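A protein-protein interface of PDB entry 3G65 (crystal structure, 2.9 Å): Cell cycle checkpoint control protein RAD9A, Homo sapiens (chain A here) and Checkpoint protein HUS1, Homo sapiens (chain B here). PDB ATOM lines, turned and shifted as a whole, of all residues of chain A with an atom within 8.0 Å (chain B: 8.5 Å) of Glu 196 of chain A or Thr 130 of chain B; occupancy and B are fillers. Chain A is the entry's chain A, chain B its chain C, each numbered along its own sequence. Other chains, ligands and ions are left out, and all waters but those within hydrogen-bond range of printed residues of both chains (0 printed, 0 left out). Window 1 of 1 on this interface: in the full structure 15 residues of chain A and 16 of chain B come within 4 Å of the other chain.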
ATOM      1  N   ALA A 155      -3.916 -24.694 -25.976  1.00  0.00           N
ATOM      2  CA  ALA A 155      -2.984 -23.577 -25.877  1.00  0.00           C
ATOM      3  C   ALA A 155      -2.172 -23.609 -24.585  1.00  0.00           C
ATOM      4  O   ALA A 155      -1.114 -22.985 -24.492  1.00  0.00           O
ATOM      5  CB  ALA A 155      -3.731 -22.255 -26.006  1.00  0.00           C
ATOM      6  N   PRO A 158       1.412 -26.980 -23.675  1.00  0.00           N
ATOM      7  CA  PRO A 158       2.873 -26.837 -23.644  1.00  0.00           C
ATOM      8  C   PRO A 158       3.403 -26.430 -22.271  1.00  0.00           C
ATOM      9  O   PRO A 158       4.594 -26.593 -22.002  1.00  0.00           O
ATOM     10  CB  PRO A 158       3.134 -25.715 -24.652  1.00  0.00           C
ATOM     11  CG  PRO A 158       1.979 -25.769 -25.580  1.00  0.00           C
ATOM     12  CD  PRO A 158       0.804 -26.159 -24.736  1.00  0.00           C
ATOM     13  N   PHE A 159       2.530 -25.904 -21.418  1.00  0.00           N
ATOM     14  CA  PHE A 159       2.938 -25.447 -20.094  1.00  0.00           C
ATOM     15  C   PHE A 159       2.954 -26.588 -19.083  1.00  0.00           C
ATOM     16  O   PHE A 159       2.142 -27.511 -19.159  1.00  0.00           O
ATOM     17  CB  PHE A 159       2.021 -24.323 -19.605  1.00  0.00           C
ATOM     18  CG  PHE A 159       2.022 -23.110 -20.492  1.00  0.00           C
ATOM     19  CD1 PHE A 159       3.132 -22.284 -20.558  1.00  0.00           C
ATOM     20  CD2 PHE A 159       0.911 -22.792 -21.255  1.00  0.00           C
ATOM     21  CE1 PHE A 159       3.134 -21.166 -21.373  1.00  0.00           C
ATOM     22  CE2 PHE A 159       0.908 -21.675 -22.070  1.00  0.00           C
ATOM     23  CZ  PHE A 159       2.020 -20.862 -22.129  1.00  0.00           C
ATOM     24  N   VAL A 166       0.677 -17.474 -15.653  1.00  0.00           N
ATOM     25  CA  VAL A 166       0.869 -17.358 -17.094  1.00  0.00           C
ATOM     26  C   VAL A 166       0.342 -16.011 -17.576  1.00  0.00           C
ATOM     27  O   VAL A 166      -0.683 -15.530 -17.096  1.00  0.00           O
ATOM     28  CB  VAL A 166       0.148 -18.490 -17.852  1.00  0.00           C
ATOM     29  CG1 VAL A 166      -1.347 -18.453 -17.571  1.00  0.00           C
ATOM     30  CG2 VAL A 166       0.421 -18.393 -19.346  1.00  0.00           C
ATOM     31  N   THR A 167       1.050 -15.399 -18.521  1.00  0.00           N
ATOM     32  CA  THR A 167       0.644 -14.098 -19.036  1.00  0.00           C
ATOM     33  C   THR A 167      -0.049 -14.224 -20.389  1.00  0.00           C
ATOM     34  O   THR A 167       0.495 -14.808 -21.326  1.00  0.00           O
ATOM     35  CB  THR A 167       1.837 -13.129 -19.166  1.00  0.00           C
ATOM     36  OG1 THR A 167       2.410 -13.240 -20.474  1.00  0.00           O
ATOM     37  CG2 THR A 167       2.896 -13.431 -18.117  1.00  0.00           C
ATOM     38  N   GLY A 171       0.284  -9.955 -29.241  1.00  0.00           N
ATOM     39  CA  GLY A 171       1.438  -9.559 -30.027  1.00  0.00           C
ATOM     40  C   GLY A 171       1.045  -8.860 -31.314  1.00  0.00           C
ATOM     41  O   GLY A 171      -0.082  -9.004 -31.791  1.00  0.00           O
ATOM     42  N   ARG A 175      -2.562 -11.660 -32.893  1.00  0.00           N
ATOM     43  CA  ARG A 175      -2.438 -13.057 -32.500  1.00  0.00           C
ATOM     44  C   ARG A 175      -2.143 -13.165 -31.007  1.00  0.00           C
ATOM     45  O   ARG A 175      -1.293 -12.448 -30.479  1.00  0.00           O
ATOM     46  CB  ARG A 175      -1.355 -13.757 -33.324  1.00  0.00           C
ATOM     47  CG  ARG A 175       0.064 -13.352 -32.972  1.00  0.00           C
ATOM     48  CD  ARG A 175       1.066 -13.949 -33.947  1.00  0.00           C
ATOM     49  NE  ARG A 175       2.419 -13.960 -33.398  1.00  0.00           N
ATOM     50  CZ  ARG A 175       3.263 -12.936 -33.465  1.00  0.00           C
ATOM     51  NH1 ARG A 175       2.896 -11.809 -34.058  1.00  0.00           N
ATOM     52  NH2 ARG A 175       4.475 -13.038 -32.936  1.00  0.00           N
ATOM     53  N   VAL A 176      -2.858 -14.057 -30.327  1.00  0.00           N
ATOM     54  CA  VAL A 176      -2.706 -14.216 -28.885  1.00  0.00           C
ATOM     55  C   VAL A 176      -1.465 -15.029 -28.538  1.00  0.00           C
ATOM     56  O   VAL A 176      -1.071 -15.930 -29.278  1.00  0.00           O
ATOM     57  CB  VAL A 176      -3.937 -14.884 -28.250  1.00  0.00           C
ATOM     58  CG1 VAL A 176      -5.211 -14.177 -28.692  1.00  0.00           C
ATOM     59  CG2 VAL A 176      -3.982 -16.357 -28.614  1.00  0.00           C
ATOM     60  N   ILE A 177      -0.858 -14.705 -27.403  1.00  0.00           N
ATOM     61  CA  ILE A 177       0.367 -15.363 -26.974  1.00  0.00           C
ATOM     62  C   ILE A 177       0.355 -15.648 -25.477  1.00  0.00           C
ATOM     63  O   ILE A 177       0.280 -14.731 -24.659  1.00  0.00           O
ATOM     64  CB  ILE A 177       1.604 -14.505 -27.295  1.00  0.00           C
ATOM     65  CG1 ILE A 177       1.697 -14.236 -28.799  1.00  0.00           C
ATOM     66  CG2 ILE A 177       2.864 -15.186 -26.789  1.00  0.00           C
ATOM     67  CD1 ILE A 177       2.837 -13.322 -29.191  1.00  0.00           C
ATOM     68  N   LEU A 178       0.430 -16.926 -25.125  1.00  0.00           N
ATOM     69  CA  LEU A 178       0.542 -17.324 -23.729  1.00  0.00           C
ATOM     70  C   LEU A 178       2.007 -17.537 -23.374  1.00  0.00           C
ATOM     71  O   LEU A 178       2.691 -18.347 -23.995  1.00  0.00           O
ATOM     72  CB  LEU A 178      -0.259 -18.600 -23.467  1.00  0.00           C
ATOM     73  CG  LEU A 178      -1.768 -18.502 -23.696  1.00  0.00           C
ATOM     74  CD1 LEU A 178      -2.413 -19.874 -23.603  1.00  0.00           C
ATOM     75  CD2 LEU A 178      -2.403 -17.537 -22.708  1.00  0.00           C
ATOM     76  N   ARG A 179       2.487 -16.800 -22.379  1.00  0.00           N
ATOM     77  CA  ARG A 179       3.883 -16.893 -21.973  1.00  0.00           C
ATOM     78  C   ARG A 179       4.004 -17.248 -20.496  1.00  0.00           C
ATOM     79  O   ARG A 179       3.274 -16.717 -19.660  1.00  0.00           O
ATOM     80  CB  ARG A 179       4.613 -15.581 -22.269  1.00  0.00           C
ATOM     81  CG  ARG A 179       6.127 -15.678 -22.193  1.00  0.00           C
ATOM     82  CD  ARG A 179       6.785 -14.429 -22.759  1.00  0.00           C
ATOM     83  NE  ARG A 179       8.240 -14.554 -22.810  1.00  0.00           N
ATOM     84  CZ  ARG A 179       9.049 -13.643 -23.343  1.00  0.00           C
ATOM     85  NH1 ARG A 179       8.546 -12.537 -23.875  1.00  0.00           N
ATOM     86  NH2 ARG A 179      10.361 -13.839 -23.346  1.00  0.00           N
ATOM     87  N   SER A 180       4.924 -18.154 -20.182  1.00  0.00           N
ATOM     88  CA  SER A 180       5.159 -18.565 -18.804  1.00  0.00           C
ATOM     89  C   SER A 180       5.689 -17.400 -17.974  1.00  0.00           C
ATOM     90  O   SER A 180       6.513 -16.615 -18.445  1.00  0.00           O
ATOM     91  CB  SER A 180       6.145 -19.733 -18.752  1.00  0.00           C
ATOM     92  OG  SER A 180       5.634 -20.859 -19.444  1.00  0.00           O
ATOM     93  N   MET A 193      12.953 -22.290 -17.546  1.00  0.00           N
ATOM     94  CA  MET A 193      12.560 -22.358 -18.949  1.00  0.00           C
ATOM     95  C   MET A 193      11.270 -21.584 -19.187  1.00  0.00           C
ATOM     96  O   MET A 193      10.276 -21.784 -18.489  1.00  0.00           O
ATOM     97  CB  MET A 193      12.401 -23.811 -19.406  1.00  0.00           C
ATOM     98  CG  MET A 193      12.000 -23.949 -20.868  1.00  0.00           C
ATOM     99  SD  MET A 193      12.069 -25.645 -21.476  1.00  0.00           S
ATOM    100  CE  MET A 193      10.896 -26.451 -20.392  1.00  0.00           C
ATOM    101  N   VAL A 194      11.294 -20.695 -20.174  1.00  0.00           N
ATOM    102  CA  VAL A 194      10.131 -19.877 -20.499  1.00  0.00           C
ATOM    103  C   VAL A 194       9.390 -20.428 -21.713  1.00  0.00           C
ATOM    104  O   VAL A 194       9.880 -20.354 -22.839  1.00  0.00           O
ATOM    105  CB  VAL A 194      10.531 -18.415 -20.770  1.00  0.00           C
ATOM    106  CG1 VAL A 194       9.313 -17.596 -21.177  1.00  0.00           C
ATOM    107  CG2 VAL A 194      11.203 -17.814 -19.544  1.00  0.00           C
ATOM    108  N   THR A 195       8.207 -20.982 -21.472  1.00  0.00           N
ATOM    109  CA  THR A 195       7.385 -21.537 -22.540  1.00  0.00           C
ATOM    110  C   THR A 195       6.465 -20.467 -23.115  1.00  0.00           C
ATOM    111  O   THR A 195       5.883 -19.675 -22.374  1.00  0.00           O
ATOM    112  CB  THR A 195       6.535 -22.719 -22.036  1.00  0.00           C
ATOM    113  OG1 THR A 195       7.393 -23.742 -21.514  1.00  0.00           O
ATOM    114  CG2 THR A 195       5.693 -23.293 -23.165  1.00  0.00           C
ATOM    115  N   GLU A 196       6.338 -20.443 -24.437  1.00  0.00           N
ATOM    116  CA  GLU A 196       5.501 -19.451 -25.099  1.00  0.00           C
ATOM    117  C   GLU A 196       4.685 -20.055 -26.234  1.00  0.00           C
ATOM    118  O   GLU A 196       5.233 -20.485 -27.248  1.00  0.00           O
ATOM    119  CB  GLU A 196       6.353 -18.290 -25.621  1.00  0.00           C
ATOM    120  CG  GLU A 196       5.581 -17.283 -26.457  1.00  0.00           C
ATOM    121  CD  GLU A 196       6.347 -15.991 -26.666  1.00  0.00           C
ATOM    122  OE1 GLU A 196       7.168 -15.638 -25.793  1.00  0.00           O
ATOM    123  OE2 GLU A 196       6.123 -15.324 -27.697  1.00  0.00           O
ATOM    124  N   MET A 197       3.370 -20.087 -26.051  1.00  0.00           N
ATOM    125  CA  MET A 197       2.463 -20.575 -27.080  1.00  0.00           C
ATOM    126  C   MET A 197       1.875 -19.411 -27.870  1.00  0.00           C
ATOM    127  O   MET A 197       1.435 -18.416 -27.293  1.00  0.00           O
ATOM    128  CB  MET A 197       1.337 -21.402 -26.457  1.00  0.00           C
ATOM    129  CG  MET A 197       0.143 -21.607 -27.379  1.00  0.00           C
ATOM    130  SD  MET A 197       0.500 -22.707 -28.762  1.00  0.00           S
ATOM    131  CE  MET A 197       0.083 -24.295 -28.045  1.00  0.00           C
ATOM    132  N   CYS A 198       1.868 -19.538 -29.191  1.00  0.00           N
ATOM    133  CA  CYS A 198       1.335 -18.495 -30.056  1.00  0.00           C
ATOM    134  C   CYS A 198       0.195 -19.019 -30.925  1.00  0.00           C
ATOM    135  O   CYS A 198       0.352 -20.009 -31.641  1.00  0.00           O
ATOM    136  CB  CYS A 198       2.446 -17.915 -30.934  1.00  0.00           C
ATOM    137  SG  CYS A 198       1.866 -16.774 -32.202  1.00  0.00           S
ATOM    138  N   LEU A 199      -0.954 -18.353 -30.856  1.00  0.00           N
ATOM    139  CA  LEU A 199      -2.118 -18.756 -31.636  1.00  0.00           C
ATOM    140  C   LEU A 199      -2.516 -17.680 -32.640  1.00  0.00           C
ATOM    141  O   LEU A 199      -2.406 -16.485 -32.361  1.00  0.00           O
ATOM    142  CB  LEU A 199      -3.302 -19.072 -30.718  1.00  0.00           C
ATOM    143  CG  LEU A 199      -3.179 -20.294 -29.805  1.00  0.00           C
ATOM    144  CD1 LEU A 199      -4.435 -20.448 -28.963  1.00  0.00           C
ATOM    145  CD2 LEU A 199      -2.923 -21.550 -30.623  1.00  0.00           C
ATOM    146  N   ALA B  91      10.101 -30.030 -23.128  1.00  0.00           N
ATOM    147  CA  ALA B  91      10.099 -29.239 -24.351  1.00  0.00           C
ATOM    148  C   ALA B  91       9.780 -30.098 -25.572  1.00  0.00           C
ATOM    149  O   ALA B  91       9.200 -29.619 -26.546  1.00  0.00           O
ATOM    150  CB  ALA B  91      11.436 -28.535 -24.530  1.00  0.00           C
ATOM    151  N   THR B  94       5.585 -31.963 -26.371  1.00  0.00           N
ATOM    152  CA  THR B  94       4.536 -31.429 -27.232  1.00  0.00           C
ATOM    153  C   THR B  94       4.862 -31.640 -28.708  1.00  0.00           C
ATOM    154  O   THR B  94       4.025 -31.400 -29.578  1.00  0.00           O
ATOM    155  CB  THR B  94       4.309 -29.928 -26.980  1.00  0.00           C
ATOM    156  OG1 THR B  94       5.545 -29.221 -27.145  1.00  0.00           O
ATOM    157  CG2 THR B  94       3.787 -29.700 -25.571  1.00  0.00           C
ATOM    158  N   LYS B 102      12.372 -27.226 -34.602  1.00  0.00           N
ATOM    159  CA  LYS B 102      13.564 -26.419 -34.834  1.00  0.00           C
ATOM    160  C   LYS B 102      14.242 -26.016 -33.530  1.00  0.00           C
ATOM    161  O   LYS B 102      13.823 -25.067 -32.868  1.00  0.00           O
ATOM    162  CB  LYS B 102      13.228 -25.174 -35.659  1.00  0.00           C
ATOM    163  CG  LYS B 102      12.760 -25.473 -37.074  1.00  0.00           C
ATOM    164  CD  LYS B 102      12.537 -24.195 -37.866  1.00  0.00           C
ATOM    165  CE  LYS B 102      12.081 -24.492 -39.286  1.00  0.00           C
ATOM    166  NZ  LYS B 102      11.925 -23.249 -40.092  1.00  0.00           N
ATOM    167  N   LYS B 108      18.639 -14.497 -26.058  1.00  0.00           N
ATOM    168  CA  LYS B 108      17.778 -13.333 -25.899  1.00  0.00           C
ATOM    169  C   LYS B 108      18.079 -12.631 -24.581  1.00  0.00           C
ATOM    170  O   LYS B 108      18.819 -11.650 -24.546  1.00  0.00           O
ATOM    171  CB  LYS B 108      16.310 -13.753 -25.949  1.00  0.00           C
ATOM    172  CG  LYS B 108      15.960 -14.634 -27.140  1.00  0.00           C
ATOM    173  CD  LYS B 108      14.578 -15.246 -26.990  1.00  0.00           C
ATOM    174  CE  LYS B 108      14.302 -16.259 -28.089  1.00  0.00           C
ATOM    175  NZ  LYS B 108      12.973 -16.911 -27.920  1.00  0.00           N
ATOM    176  N   HIS B 109      17.500 -13.140 -23.499  1.00  0.00           N
ATOM    177  CA  HIS B 109      17.763 -12.604 -22.169  1.00  0.00           C
ATOM    178  C   HIS B 109      19.048 -13.201 -21.614  1.00  0.00           C
ATOM    179  O   HIS B 109      19.898 -12.490 -21.079  1.00  0.00           O
ATOM    180  CB  HIS B 109      16.593 -12.908 -21.232  1.00  0.00           C
ATOM    181  CG  HIS B 109      15.289 -12.335 -21.690  1.00  0.00           C
ATOM    182  ND1 HIS B 109      14.794 -11.141 -21.214  1.00  0.00           N
ATOM    183  CD2 HIS B 109      14.379 -12.790 -22.584  1.00  0.00           C
ATOM    184  CE1 HIS B 109      13.634 -10.885 -21.792  1.00  0.00           C
ATOM    185  NE2 HIS B 109      13.360 -11.871 -22.628  1.00  0.00           N
ATOM    186  N   LEU B 113      18.620 -22.505 -25.159  1.00  0.00           N
ATOM    187  CA  LEU B 113      18.508 -23.408 -26.294  1.00  0.00           C
ATOM    188  C   LEU B 113      17.053 -23.472 -26.740  1.00  0.00           C
ATOM    189  O   LEU B 113      16.309 -24.370 -26.344  1.00  0.00           O
ATOM    190  CB  LEU B 113      19.015 -24.802 -25.917  1.00  0.00           C
ATOM    191  CG  LEU B 113      19.163 -25.824 -27.043  1.00  0.00           C
ATOM    192  CD1 LEU B 113      20.065 -25.284 -28.138  1.00  0.00           C
ATOM    193  CD2 LEU B 113      19.712 -27.129 -26.495  1.00  0.00           C
ATOM    194  N   THR B 114      16.652 -22.505 -27.561  1.00  0.00           N
ATOM    195  CA  THR B 114      15.262 -22.383 -27.992  1.00  0.00           C
ATOM    196  C   THR B 114      14.794 -23.582 -28.806  1.00  0.00           C
ATOM    197  O   THR B 114      15.409 -23.948 -29.805  1.00  0.00           O
ATOM    198  CB  THR B 114      15.028 -21.100 -28.813  1.00  0.00           C
ATOM    199  OG1 THR B 114      15.251 -19.953 -27.984  1.00  0.00           O
ATOM    200  CG2 THR B 114      13.603 -21.059 -29.338  1.00  0.00           C
ATOM    201  N   VAL B 115      13.693 -24.183 -28.370  1.00  0.00           N
ATOM    202  CA  VAL B 115      13.106 -25.312 -29.075  1.00  0.00           C
ATOM    203  C   VAL B 115      11.759 -24.914 -29.665  1.00  0.00           C
ATOM    204  O   VAL B 115      10.717 -25.086 -29.031  1.00  0.00           O
ATOM    205  CB  VAL B 115      12.914 -26.519 -28.140  1.00  0.00           C
ATOM    206  CG1 VAL B 115      12.317 -27.696 -28.901  1.00  0.00           C
ATOM    207  CG2 VAL B 115      14.237 -26.903 -27.491  1.00  0.00           C
ATOM    208  N   SER B 116      11.788 -24.369 -30.876  1.00  0.00           N
ATOM    209  CA  SER B 116      10.566 -23.960 -31.555  1.00  0.00           C
ATOM    210  C   SER B 116       9.853 -25.167 -32.157  1.00  0.00           C
ATOM    211  O   SER B 116      10.478 -26.025 -32.779  1.00  0.00           O
ATOM    212  CB  SER B 116      10.874 -22.935 -32.646  1.00  0.00           C
ATOM    213  OG  SER B 116      11.692 -23.497 -33.657  1.00  0.00           O
ATOM    214  N   VAL B 117       8.539 -25.224 -31.965  1.00  0.00           N
ATOM    215  CA  VAL B 117       7.742 -26.340 -32.458  1.00  0.00           C
ATOM    216  C   VAL B 117       6.552 -25.847 -33.273  1.00  0.00           C
ATOM    217  O   VAL B 117       5.842 -24.932 -32.858  1.00  0.00           O
ATOM    218  CB  VAL B 117       7.222 -27.211 -31.299  1.00  0.00           C
ATOM    219  CG1 VAL B 117       6.494 -28.432 -31.839  1.00  0.00           C
ATOM    220  CG2 VAL B 117       8.368 -27.625 -30.388  1.00  0.00           C
ATOM    221  N   GLU B 118       6.337 -26.455 -34.433  1.00  0.00           N
ATOM    222  CA  GLU B 118       5.183 -26.124 -35.259  1.00  0.00           C
ATOM    223  C   GLU B 118       4.124 -27.217 -35.170  1.00  0.00           C
ATOM    224  O   GLU B 118       4.316 -28.324 -35.673  1.00  0.00           O
ATOM    225  CB  GLU B 118       5.597 -25.909 -36.716  1.00  0.00           C
ATOM    226  CG  GLU B 118       4.431 -25.614 -37.648  1.00  0.00           C
ATOM    227  CD  GLU B 118       4.871 -25.343 -39.072  1.00  0.00           C
ATOM    228  OE1 GLU B 118       6.089 -25.173 -39.298  1.00  0.00           O
ATOM    229  OE2 GLU B 118       3.998 -25.298 -39.966  1.00  0.00           O
ATOM    230  N   LEU B 119       3.007 -26.900 -34.522  1.00  0.00           N
ATOM    231  CA  LEU B 119       1.914 -27.852 -34.371  1.00  0.00           C
ATOM    232  C   LEU B 119       0.819 -27.574 -35.394  1.00  0.00           C
ATOM    233  O   LEU B 119       0.279 -26.470 -35.451  1.00  0.00           O
ATOM    234  CB  LEU B 119       1.339 -27.781 -32.956  1.00  0.00           C
ATOM    235  CG  LEU B 119       2.334 -27.983 -31.813  1.00  0.00           C
ATOM    236  CD1 LEU B 119       1.674 -27.729 -30.465  1.00  0.00           C
ATOM    237  CD2 LEU B 119       2.931 -29.380 -31.869  1.00  0.00           C
ATOM    238  N   ARG B 127       0.146 -23.305 -35.464  1.00  0.00           N
ATOM    239  CA  ARG B 127       0.402 -23.175 -34.034  1.00  0.00           C
ATOM    240  C   ARG B 127       1.900 -23.245 -33.770  1.00  0.00           C
ATOM    241  O   ARG B 127       2.598 -24.083 -34.342  1.00  0.00           O
ATOM    242  CB  ARG B 127      -0.308 -24.286 -33.258  1.00  0.00           C
ATOM    243  CG  ARG B 127      -1.686 -24.647 -33.789  1.00  0.00           C
ATOM    244  CD  ARG B 127      -2.688 -23.528 -33.572  1.00  0.00           C
ATOM    245  NE  ARG B 127      -4.037 -23.932 -33.958  1.00  0.00           N
ATOM    246  CZ  ARG B 127      -4.871 -24.601 -33.167  1.00  0.00           C
ATOM    247  NH1 ARG B 127      -4.495 -24.943 -31.943  1.00  0.00           N
ATOM    248  NH2 ARG B 127      -6.080 -24.929 -33.601  1.00  0.00           N
ATOM    249  N   ILE B 128       2.393 -22.366 -32.903  1.00  0.00           N
ATOM    250  CA  ILE B 128       3.819 -22.327 -32.597  1.00  0.00           C
ATOM    251  C   ILE B 128       4.094 -22.320 -31.094  1.00  0.00           C
ATOM    252  O   ILE B 128       3.542 -21.507 -30.353  1.00  0.00           O
ATOM    253  CB  ILE B 128       4.502 -21.108 -33.238  1.00  0.00           C
ATOM    254  CG1 ILE B 128       4.248 -21.088 -34.747  1.00  0.00           C
ATOM    255  CG2 ILE B 128       5.994 -21.122 -32.943  1.00  0.00           C
ATOM    256  CD1 ILE B 128       4.752 -19.841 -35.432  1.00  0.00           C
ATOM    257  N   VAL B 129       4.953 -23.233 -30.656  1.00  0.00           N
ATOM    258  CA  VAL B 129       5.349 -23.307 -29.257  1.00  0.00           C
ATOM    259  C   VAL B 129       6.863 -23.207 -29.130  1.00  0.00           C
ATOM    260  O   VAL B 129       7.591 -24.066 -29.628  1.00  0.00           O
ATOM    261  CB  VAL B 129       4.894 -24.622 -28.611  1.00  0.00           C
ATOM    262  CG1 VAL B 129       5.322 -24.665 -27.155  1.00  0.00           C
ATOM    263  CG2 VAL B 129       3.392 -24.781 -28.736  1.00  0.00           C
ATOM    264  N   THR B 130       7.337 -22.159 -28.465  1.00  0.00           N
ATOM    265  CA  THR B 130       8.770 -21.963 -28.283  1.00  0.00           C
ATOM    266  C   THR B 130       9.177 -22.166 -26.827  1.00  0.00           C
ATOM    267  O   THR B 130       8.564 -21.608 -25.916  1.00  0.00           O
ATOM    268  CB  THR B 130       9.213 -20.560 -28.730  1.00  0.00           C
ATOM    269  OG1 THR B 130       8.720 -19.584 -27.803  1.00  0.00           O
ATOM    270  CG2 THR B 130       8.683 -20.250 -30.122  1.00  0.00           C
ATOM    271  N   HIS B 131      10.213 -22.969 -26.616  1.00  0.00           N
ATOM    272  CA  HIS B 131      10.738 -23.206 -25.279  1.00  0.00           C
ATOM    273  C   HIS B 131      12.153 -22.650 -25.159  1.00  0.00           C
ATOM    274  O   HIS B 131      13.008 -22.919 -26.002  1.00  0.00           O
ATOM    275  CB  HIS B 131      10.739 -24.702 -24.956  1.00  0.00           C
ATOM    276  CG  HIS B 131       9.386 -25.340 -25.029  1.00  0.00           C
ATOM    277  ND1 HIS B 131       8.549 -25.437 -23.940  1.00  0.00           N
ATOM    278  CD2 HIS B 131       8.730 -25.922 -26.062  1.00  0.00           C
ATOM    279  CE1 HIS B 131       7.434 -26.048 -24.297  1.00  0.00           C
ATOM    280  NE2 HIS B 131       7.518 -26.353 -25.580  1.00  0.00           N
ATOM    281  N   ASP B 132      12.395 -21.870 -24.110  1.00  0.00           N
ATOM    282  CA  ASP B 132      13.721 -21.318 -23.860  1.00  0.00           C
ATOM    283  C   ASP B 132      14.435 -22.100 -22.763  1.00  0.00           C
ATOM    284  O   ASP B 132      14.313 -21.780 -21.581  1.00  0.00           O
ATOM    285  CB  ASP B 132      13.624 -19.841 -23.478  1.00  0.00           C
ATOM    286  CG  ASP B 132      13.221 -18.963 -24.646  1.00  0.00           C
ATOM    287  OD1 ASP B 132      13.713 -19.202 -25.768  1.00  0.00           O
ATOM    288  OD2 ASP B 132      12.416 -18.029 -24.441  1.00  0.00           O
ATOM    289  N   ILE B 133      15.179 -23.125 -23.163  1.00  0.00           N
ATOM    290  CA  ILE B 133      15.915 -23.957 -22.217  1.00  0.00           C
ATOM    291  C   ILE B 133      17.206 -23.283 -21.768  1.00  0.00           C
ATOM    292  O   ILE B 133      18.129 -23.111 -22.563  1.00  0.00           O
ATOM    293  CB  ILE B 133      16.264 -25.328 -22.826  1.00  0.00           C
ATOM    294  CG1 ILE B 133      15.001 -26.032 -23.326  1.00  0.00           C
ATOM    295  CG2 ILE B 133      16.997 -26.188 -21.808  1.00  0.00           C
ATOM    296  CD1 ILE B 133      15.263 -27.387 -23.949  1.00  0.00           C
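O of Val 194 of chain A lies within hydrogen-bond range of N of Asp 132 of chain B.
ND1 of His 131 of chain B lies within hydrogen-bond range of OG1 of Thr 195 of chain A (3.2 Å).
The backbone NH of Glu 196 of chain A lies within hydrogen-bond range of the backbone carbonyl oxygen of Thr 130 of chain B.
O of Ile 128 of chain B lies within hydrogen-bond range of N of Cys 198 of chain A, at 2.8 Å.
SD of Met 197 of chain A lies close to O of Ile 128 of chain B (3.6 Å).
NE of Arg 175 of chain A lies within hydrogen-bond range of SG of Cys 198 of chain A, at 3.1 Å.
The backbone carbonyl oxygen (O) of Thr 195 of chain A sits at hydrogen-bond distance from the backbone NH (N) of Ser 180 of chain A (2.8 Å).
The backbone NH of Leu 113 of chain B is in hydrogen-bond range of the backbone carbonyl oxygen of Ile 133 of chain B.
The side-chain carboxylate (OD1) of Asp 132 of chain B lies within hydrogen-bond range of the side-chain hydroxyl (OG1) of Thr 114 of chain B.
The backbone carbonyl oxygen (O) of His 131 of chain B sits at hydrogen-bond distance from the backbone NH (N) of Val 115 of chain B (2.8 Å).
The backbone carbonyl oxygen (O) of Val 129 of chain B is in hydrogen-bond range of the backbone NH (N) of Val 117 of chain B (2.8 Å).
Among the printed residues, merely in contact across the chains: Met 193 of chain A with Asp 132 of chain B, Met 197 of chain A with Val 129 of chain B, Glu 196 of chain A with Val 129 of chain B, Pro 158 of chain A with Val 129 of chain B, Met 193 of chain A with Ile 133 of chain B, Leu 199 of chain A with Arg 127 of chain B, Pro 158 of chain A with Thr 94 of chain B, Val 194 of chain A with Thr 130 of chain B, Thr 195 of chain A with Thr 130 of chain B, Arg 179 of chain A with His 109 of chain B, Glu 196 of chain A with Ile 128 of chain B, Pro 158 of chain A with His 131 of chain B, Met 193 of chain A with His 131 of chain B, Val 194 of chain A with His 131 of chain B and Cys 198 of chain A with Arg 127 of chain B.
Ala 155 of chain A touches none of the printed residues of chain B.
Printed residues of chain B within 4 Å of Val 194 of chain A: Thr 130 (3.6 Å), His 131 (3.9 Å) and Asp 132 (3.2 Å).
Of chain B, only Ile 128, Val 129 and Thr 130 come within 4 Å of Glu 196 of chain A.
Printed residues of chain B within 4 Å of Met 197 of chain A: Ile 128 and Val 129.
Leu 119 of chain B touches none of the printed residues of chain A.
Thr 130 of chain B touches three residues of chain A.
Printed residues of chain A within 4 Å of Ile 133 of chain B: Met 193 (3.5 Å).
The nearest residue of chain B that does not touch Glu 196 of chain A is His 131 of chain B (5.1 Å).
The nearest residue of chain A that does not touch Thr 130 of chain B is Met 197 of chain A (5.1 Å).
The nearest printed residue of chain B that does not touch Leu 199 of chain A is Ile 128 of chain B (5.5 Å).
Printed residues of chain B that touch a printed residue of chain A: Thr 94, His 109, Arg 127, Ile 128, Val 129, Thr 130, His 131, Asp 132 and Ile 133.
Hydrophobic or aromatic side chains of chain B within 4 Å of the printed part of chain A: His 109, Val 129, His 131 and Ile 133.
Along chain B the printed residues that touch a printed residue of chain A span positions 94 to 133.
Among the printed residues, 20 pairs touch across the chains.
Among the printed residues, no Asp or Glu carboxylate lies within 4 Å of a Lys or Arg side-chain nitrogen of the other chain.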
